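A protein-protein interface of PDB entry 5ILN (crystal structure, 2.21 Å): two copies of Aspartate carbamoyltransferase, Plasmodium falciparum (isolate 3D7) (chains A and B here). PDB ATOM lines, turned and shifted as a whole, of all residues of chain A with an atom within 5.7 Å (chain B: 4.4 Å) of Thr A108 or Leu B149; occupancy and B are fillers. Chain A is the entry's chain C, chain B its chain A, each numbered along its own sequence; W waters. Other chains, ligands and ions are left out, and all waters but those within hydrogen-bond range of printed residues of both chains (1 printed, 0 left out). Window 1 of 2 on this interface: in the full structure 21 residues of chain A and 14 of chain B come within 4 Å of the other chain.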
ATOM      1  N   PRO A 106     -38.272  12.350  -0.722  1.00  0.00           N
ATOM      2  CA  PRO A 106     -36.939  11.798  -0.999  1.00  0.00           C
ATOM      3  C   PRO A 106     -35.878  12.182   0.048  1.00  0.00           C
ATOM      4  O   PRO A 106     -35.875  13.308   0.594  1.00  0.00           O
ATOM      5  CB  PRO A 106     -36.632  12.354  -2.399  1.00  0.00           C
ATOM      6  CG  PRO A 106     -37.970  12.575  -3.036  1.00  0.00           C
ATOM      7  CD  PRO A 106     -38.799  13.084  -1.906  1.00  0.00           C
ATOM      8  N   SER A 107     -35.039  11.235   0.367  1.00  0.00           N
ATOM      9  CA  SER A 107     -33.912  11.495   1.283  1.00  0.00           C
ATOM     10  C   SER A 107     -32.755  10.516   1.156  1.00  0.00           C
ATOM     11  O   SER A 107     -32.980   9.349   1.040  1.00  0.00           O
ATOM     12  CB  SER A 107     -34.397  11.445   2.704  1.00  0.00           C
ATOM     13  OG  SER A 107     -33.276  11.624   3.591  1.00  0.00           O
ATOM     14  N   THR A 108     -31.501  10.999   1.211  1.00  0.00           N
ATOM     15  CA  THR A 108     -30.329  10.134   1.371  1.00  0.00           C
ATOM     16  C   THR A 108     -29.681  10.273   2.781  1.00  0.00           C
ATOM     17  O   THR A 108     -29.619   9.303   3.572  1.00  0.00           O
ATOM     18  CB  THR A 108     -29.304  10.352   0.248  1.00  0.00           C
ATOM     19  OG1 THR A 108     -29.896  10.040  -1.027  1.00  0.00           O
ATOM     20  CG2 THR A 108     -28.109   9.402   0.399  1.00  0.00           C
ATOM     21  N   ARG A 109     -29.166  11.469   3.058  1.00  0.00           N
ATOM     22  CA  ARG A 109     -28.357  11.642   4.208  1.00  0.00           C
ATOM     23  C   ARG A 109     -29.236  11.340   5.386  1.00  0.00           C
ATOM     24  O   ARG A 109     -28.833  10.595   6.241  1.00  0.00           O
ATOM     25  CB  ARG A 109     -27.886  13.070   4.348  1.00  0.00           C
ATOM     26  CG  ARG A 109     -26.524  13.404   3.741  1.00  0.00           C
ATOM     27  CD  ARG A 109     -26.618  14.881   3.225  1.00  0.00           C
ATOM     28  NE  ARG A 109     -27.577  14.825   2.133  1.00  0.00           N
ATOM     29  CZ  ARG A 109     -27.283  14.379   0.905  1.00  0.00           C
ATOM     30  NH1 ARG A 109     -28.278  14.266   0.040  1.00  0.00           N
ATOM     31  NH2 ARG A 109     -25.986  14.150   0.542  1.00  0.00           N
ATOM     32  N   THR A 110     -30.427  11.921   5.415  1.00  0.00           N
ATOM     33  CA  THR A 110     -31.212  11.955   6.619  1.00  0.00           C
ATOM     34  C   THR A 110     -31.760  10.556   6.909  1.00  0.00           C
ATOM     35  O   THR A 110     -31.647  10.097   8.040  1.00  0.00           O
ATOM     36  CB  THR A 110     -32.381  12.961   6.575  1.00  0.00           C
ATOM     37  OG1 THR A 110     -31.873  14.271   6.253  1.00  0.00           O
ATOM     38  CG2 THR A 110     -33.119  13.047   7.877  1.00  0.00           C
ATOM     39  N   ARG A 111     -32.403   9.950   5.909  1.00  0.00           N
ATOM     40  CA  ARG A 111     -32.934   8.626   6.073  1.00  0.00           C
ATOM     41  C   ARG A 111     -31.873   7.621   6.358  1.00  0.00           C
ATOM     42  O   ARG A 111     -32.024   6.815   7.252  1.00  0.00           O
ATOM     43  CB  ARG A 111     -33.645   8.234   4.789  1.00  0.00           C
ATOM     44  CG  ARG A 111     -34.323   6.851   4.893  1.00  0.00           C
ATOM     45  CD  ARG A 111     -35.282   6.637   3.777  1.00  0.00           C
ATOM     46  NE  ARG A 111     -34.743   6.872   2.416  1.00  0.00           N
ATOM     47  CZ  ARG A 111     -34.467   5.910   1.533  1.00  0.00           C
ATOM     48  NH1 ARG A 111     -33.971   6.228   0.334  1.00  0.00           N
ATOM     49  NH2 ARG A 111     -34.686   4.618   1.825  1.00  0.00           N
ATOM     50  N   CSO A 112     -30.805   7.621   5.554  1.00  0.00           N
ATOM     51  CA  CSO A 112     -29.760   6.575   5.701  1.00  0.00           C
ATOM     52  CB  CSO A 112     -28.827   6.397   4.473  1.00  0.00           C
ATOM     53  SG  CSO A 112     -29.587   6.035   2.919  1.00  0.00           S
ATOM     54  C   CSO A 112     -28.973   6.740   7.013  1.00  0.00           C
ATOM     55  O   CSO A 112     -28.530   5.780   7.640  1.00  0.00           O
ATOM     56  OD  CSO A 112     -29.859   4.217   3.176  1.00  0.00           O
ATOM     57  N   SER A 113     -28.774   7.959   7.432  1.00  0.00           N
ATOM     58  CA  SER A 113     -27.986   8.181   8.610  1.00  0.00           C
ATOM     59  C   SER A 113     -28.784   7.835   9.868  1.00  0.00           C
ATOM     60  O   SER A 113     -28.197   7.385  10.833  1.00  0.00           O
ATOM     61  CB  SER A 113     -27.465   9.643   8.687  1.00  0.00           C
ATOM     62  OG  SER A 113     -28.488  10.552   9.002  1.00  0.00           O
ATOM     63  N   CYS B 100     -24.498  -0.978   2.837  1.00  0.00           N
ATOM     64  CA  CYS B 100     -25.532  -0.272   2.091  1.00  0.00           C
ATOM     65  C   CYS B 100     -25.610  -1.029   0.831  1.00  0.00           C
ATOM     66  O   CYS B 100     -24.634  -1.172   0.212  1.00  0.00           O
ATOM     67  CB  CYS B 100     -25.156   1.251   1.755  1.00  0.00           C
ATOM     68  SG  CYS B 100     -26.620   2.166   1.095  1.00  0.00           S
ATOM     69  N   THR B 134     -34.680   8.823  -3.004  1.00  0.00           N
ATOM     70  CA  THR B 134     -33.318   9.188  -2.730  1.00  0.00           C
ATOM     71  C   THR B 134     -33.088  10.681  -3.187  1.00  0.00           C
ATOM     72  O   THR B 134     -33.855  11.244  -3.981  1.00  0.00           O
ATOM     73  CB  THR B 134     -32.495   8.175  -3.574  1.00  0.00           C
ATOM     74  OG1 THR B 134     -32.052   7.044  -2.767  1.00  0.00           O
ATOM     75  CG2 THR B 134     -31.465   8.798  -4.217  1.00  0.00           C
ATOM     76  N   SER B 135     -32.043  11.305  -2.653  1.00  0.00           N
ATOM     77  CA  SER B 135     -31.644  12.655  -3.067  1.00  0.00           C
ATOM     78  C   SER B 135     -31.092  12.754  -4.508  1.00  0.00           C
ATOM     79  O   SER B 135     -30.993  13.867  -5.069  1.00  0.00           O
ATOM     80  CB  SER B 135     -30.767  13.349  -2.006  1.00  0.00           C
ATOM     81  OG  SER B 135     -31.654  13.858  -0.975  1.00  0.00           O
ATOM     82  N   GLU B 140     -28.623  15.128  -7.018  1.00  0.00           N
ATOM     83  CA  GLU B 140     -27.325  14.930  -6.382  1.00  0.00           C
ATOM     84  C   GLU B 140     -26.464  14.100  -7.314  1.00  0.00           C
ATOM     85  O   GLU B 140     -26.992  13.208  -7.877  1.00  0.00           O
ATOM     86  CB  GLU B 140     -27.449  14.162  -5.053  1.00  0.00           C
ATOM     87  CG  GLU B 140     -26.114  13.891  -4.348  1.00  0.00           C
ATOM     88  CD  GLU B 140     -26.229  13.758  -2.834  1.00  0.00           C
ATOM     89  OE1 GLU B 140     -27.263  13.236  -2.313  1.00  0.00           O
ATOM     90  OE2 GLU B 140     -25.285  14.188  -2.115  1.00  0.00           O
ATOM     91  N   ALA B 145     -23.002  11.554  -3.402  1.00  0.00           N
ATOM     92  CA  ALA B 145     -23.808  10.551  -2.710  1.00  0.00           C
ATOM     93  C   ALA B 145     -22.959   9.425  -2.159  1.00  0.00           C
ATOM     94  O   ALA B 145     -23.140   9.056  -1.029  1.00  0.00           O
ATOM     95  CB  ALA B 145     -24.880   9.998  -3.627  1.00  0.00           C
ATOM     96  N   PHE B 146     -21.972   8.948  -2.919  1.00  0.00           N
ATOM     97  CA  PHE B 146     -21.091   7.872  -2.441  1.00  0.00           C
ATOM     98  C   PHE B 146     -20.028   8.314  -1.414  1.00  0.00           C
ATOM     99  O   PHE B 146     -19.645   7.549  -0.511  1.00  0.00           O
ATOM    100  CB  PHE B 146     -20.504   7.036  -3.636  1.00  0.00           C
ATOM    101  CG  PHE B 146     -21.500   6.147  -4.220  1.00  0.00           C
ATOM    102  CD1 PHE B 146     -22.461   6.662  -5.059  1.00  0.00           C
ATOM    103  CD2 PHE B 146     -21.611   4.815  -3.779  1.00  0.00           C
ATOM    104  CE1 PHE B 146     -23.434   5.903  -5.596  1.00  0.00           C
ATOM    105  CE2 PHE B 146     -22.643   4.015  -4.259  1.00  0.00           C
ATOM    106  CZ  PHE B 146     -23.567   4.546  -5.163  1.00  0.00           C
ATOM    107  N   LYS B 147     -19.545   9.534  -1.544  1.00  0.00           N
ATOM    108  CA  LYS B 147     -18.589  10.073  -0.582  1.00  0.00           C
ATOM    109  C   LYS B 147     -19.206  10.018   0.838  1.00  0.00           C
ATOM    110  O   LYS B 147     -18.613   9.573   1.800  1.00  0.00           O
ATOM    111  CB  LYS B 147     -18.231  11.491  -0.985  1.00  0.00           C
ATOM    112  CG  LYS B 147     -17.057  12.088  -0.266  1.00  0.00           C
ATOM    113  CD  LYS B 147     -16.116  12.670  -1.341  1.00  0.00           C
ATOM    114  CE  LYS B 147     -14.976  13.515  -0.779  1.00  0.00           C
ATOM    115  NZ  LYS B 147     -14.431  13.002   0.497  1.00  0.00           N
ATOM    116  N   ILE B 148     -20.448  10.370   0.881  1.00  0.00           N
ATOM    117  CA  ILE B 148     -21.270  10.405   2.096  1.00  0.00           C
ATOM    118  C   ILE B 148     -21.718   8.995   2.623  1.00  0.00           C
ATOM    119  O   ILE B 148     -21.502   8.676   3.791  1.00  0.00           O
ATOM    120  CB  ILE B 148     -22.493  11.360   1.813  1.00  0.00           C
ATOM    121  CG1 ILE B 148     -21.963  12.774   1.640  1.00  0.00           C
ATOM    122  CG2 ILE B 148     -23.515  11.368   2.955  1.00  0.00           C
ATOM    123  CD1 ILE B 148     -22.971  13.836   1.343  1.00  0.00           C
ATOM    124  N   LEU B 149     -22.331   8.187   1.752  1.00  0.00           N
ATOM    125  CA  LEU B 149     -22.761   6.830   2.098  1.00  0.00           C
ATOM    126  C   LEU B 149     -21.625   5.990   2.666  1.00  0.00           C
ATOM    127  O   LEU B 149     -21.827   5.268   3.643  1.00  0.00           O
ATOM    128  CB  LEU B 149     -23.391   6.129   0.927  1.00  0.00           C
ATOM    129  CG  LEU B 149     -24.786   6.577   0.434  1.00  0.00           C
ATOM    130  CD1 LEU B 149     -24.995   6.112  -1.009  1.00  0.00           C
ATOM    131  CD2 LEU B 149     -25.998   6.144   1.291  1.00  0.00           C
ATOM    132  N   SER B 150     -20.453   6.104   2.070  1.00  0.00           N
ATOM    133  CA  SER B 150     -19.232   5.529   2.586  1.00  0.00           C
ATOM    134  C   SER B 150     -18.984   5.794   4.031  1.00  0.00           C
ATOM    135  O   SER B 150     -18.332   5.010   4.712  1.00  0.00           O
ATOM    136  CB  SER B 150     -18.063   6.283   2.015  1.00  0.00           C
ATOM    137  OG  SER B 150     -17.803   5.969   0.729  1.00  0.00           O
ATOM    138  N   THR B 151     -19.368   6.960   4.500  1.00  0.00           N
ATOM    139  CA  THR B 151     -19.087   7.252   5.947  1.00  0.00           C
ATOM    140  C   THR B 151     -20.111   6.598   6.913  1.00  0.00           C
ATOM    141  O   THR B 151     -19.819   6.431   8.044  1.00  0.00           O
ATOM    142  CB  THR B 151     -19.037   8.776   6.273  1.00  0.00           C
ATOM    143  OG1 THR B 151     -20.267   9.379   5.842  1.00  0.00           O
ATOM    144  CG2 THR B 151     -17.789   9.443   5.644  1.00  0.00           C
ATOM    145  N   TYR B 152     -21.281   6.206   6.449  1.00  0.00           N
ATOM    146  CA  TYR B 152     -22.220   5.586   7.321  1.00  0.00           C
ATOM    147  C   TYR B 152     -22.050   4.063   7.519  1.00  0.00           C
ATOM    148  O   TYR B 152     -22.595   3.497   8.469  1.00  0.00           O
ATOM    149  CB  TYR B 152     -23.581   5.823   6.702  1.00  0.00           C
ATOM    150  CG  TYR B 152     -24.007   7.228   6.467  1.00  0.00           C
ATOM    151  CD1 TYR B 152     -23.675   8.250   7.345  1.00  0.00           C
ATOM    152  CD2 TYR B 152     -24.837   7.536   5.395  1.00  0.00           C
ATOM    153  CE1 TYR B 152     -24.130   9.567   7.129  1.00  0.00           C
ATOM    154  CE2 TYR B 152     -25.313   8.814   5.207  1.00  0.00           C
ATOM    155  CZ  TYR B 152     -24.965   9.836   6.044  1.00  0.00           C
ATOM    156  OH  TYR B 152     -25.471  11.136   5.832  1.00  0.00           O
ATOM    157  N   VAL B 153     -21.361   3.412   6.574  1.00  0.00           N
ATOM    158  CA  VAL B 153     -21.263   1.959   6.455  1.00  0.00           C
ATOM    159  C   VAL B 153     -19.868   1.403   6.176  1.00  0.00           C
ATOM    160  O   VAL B 153     -19.002   2.153   5.711  1.00  0.00           O
ATOM    161  CB  VAL B 153     -22.171   1.493   5.312  1.00  0.00           C
ATOM    162  CG1 VAL B 153     -23.591   2.027   5.496  1.00  0.00           C
ATOM    163  CG2 VAL B 153     -21.692   1.914   3.951  1.00  0.00           C
ATOM    164  N   ILE B 156     -20.368  -1.447   0.403  1.00  0.00           N
ATOM    165  CA  ILE B 156     -21.435  -1.034  -0.485  1.00  0.00           C
ATOM    166  C   ILE B 156     -21.591  -2.014  -1.589  1.00  0.00           C
ATOM    167  O   ILE B 156     -20.612  -2.323  -2.255  1.00  0.00           O
ATOM    168  CB  ILE B 156     -21.129   0.377  -1.082  1.00  0.00           C
ATOM    169  CG1 ILE B 156     -21.268   1.407   0.040  1.00  0.00           C
ATOM    170  CG2 ILE B 156     -22.120   0.752  -2.167  1.00  0.00           C
ATOM    171  CD1 ILE B 156     -20.973   2.884  -0.324  1.00  0.00           C
HETATM  172  O   HOH W   1     -28.438  10.632  -3.164  1.00  0.00           O
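Along chain B the printed residues that touch a printed residue of chain A span positions 134 to 152. Of the 8 printed residues of chain A, 7 touch a printed residue of chain B. Hydrophobic or aromatic side chains of chain A that line the printed part of chain B: Pro A106. Among the printed residues, 13 pairs touch across the chains. Among the printed residues, Asp or Glu carboxylates within 4 Å of a Lys or Arg side-chain nitrogen of the other chain: Arg A109 with Glu B140.
Water W1 lies within hydrogen-bond range of the side-chain hydroxyl (OG1) of Thr A108 and the side-chain carboxylate (OE1) of Glu B140.
The backbone carbonyl oxygen (O) of Ile B148 lies within hydrogen-bond range of the side-chain hydroxyl (OG1) of Thr B151, at 2.5 Å. OG of Ser A113 lies within hydrogen-bond range of O of Thr A110 (3.3 Å). The backbone carbonyl oxygen of Ser B135 lies within hydrogen-bond range of the backbone NH of Glu B140, 3.3 Å away. O of Arg A109 lies within hydrogen-bond range of OG of Ser A113, at 2.8 Å. OG of Ser A107 lies within hydrogen-bond range of N of Arg A111. The backbone NH (N) of Thr A110 sits close to the side-chain hydroxyl (OG) of Ser A107 (3.4 Å).
Of the printed residues of chain B, Thr A108 touches Thr B134 (3.8 Å), Ser B135 (3.0 Å) and Leu B149 (3.98 Å). Printed residues of chain A within 4 Å of Leu B149: Thr A108 and CSO A112. Of the printed residues of chain B, Ser A113 touches Tyr B152. Of the printed residues of chain A, Ser B135 touches Ser A107 (3.95 Å), Thr A108 (3.0 Å) and Arg A109 (3.3 Å). Printed residues of chain B within 4 Å of Pro A106: Thr B134 (3.4 Å). Of the printed residues of chain B, Ser A107 touches Thr B134 (3.8 Å) and Ser B135 (3.95 Å). Printed residues of chain A within 4 Å of Ile B148: Arg A109. Lys B147 touches none of the printed residues of chain A. Phe B146 touches none of the printed residues of chain A. The nearest printed residue of chain B that does not touch Thr A108 is Glu B140 (4.3 Å).
No position is printed for both chains. Of the 13 pairs that touch across the chains among the printed residues, none has its exchanged pair printed and touching as well.
OH of Tyr B152 sits close to O of Arg A109. The side-chain carboxylate (OE2) of Glu B140 lies within salt-bridge range of the guanidinium group (NH2) of Arg A109 (2.7 Å). N of Ser B135 sits at hydrogen-bond distance from OG1 of Thr A108.
O of Thr B134 touches CB of Pro A106, 3.4 Å away. CA of Thr B134 touches O of Ser A107, 3.8 Å away. Ser A107 touches Ser B135. Thr B134 touches Thr A108 (CG2 to OG1, 3.8 Å). CG2 of Thr A108 touches CD2 of Leu B149, at 3.98 Å. Arg A109 touches Ser B135 (NH1 to CB, 3.3 Å). Arg A109 touches Ile B148. Thr B134 touches Arg A111 (OG1 to NH1, 3.7 Å). SG of CSO A112 touches CD2 of Leu B149, at 3.9 Å. Tyr B152 touches Ser A113 (CZ to CB, 3.6 Å).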
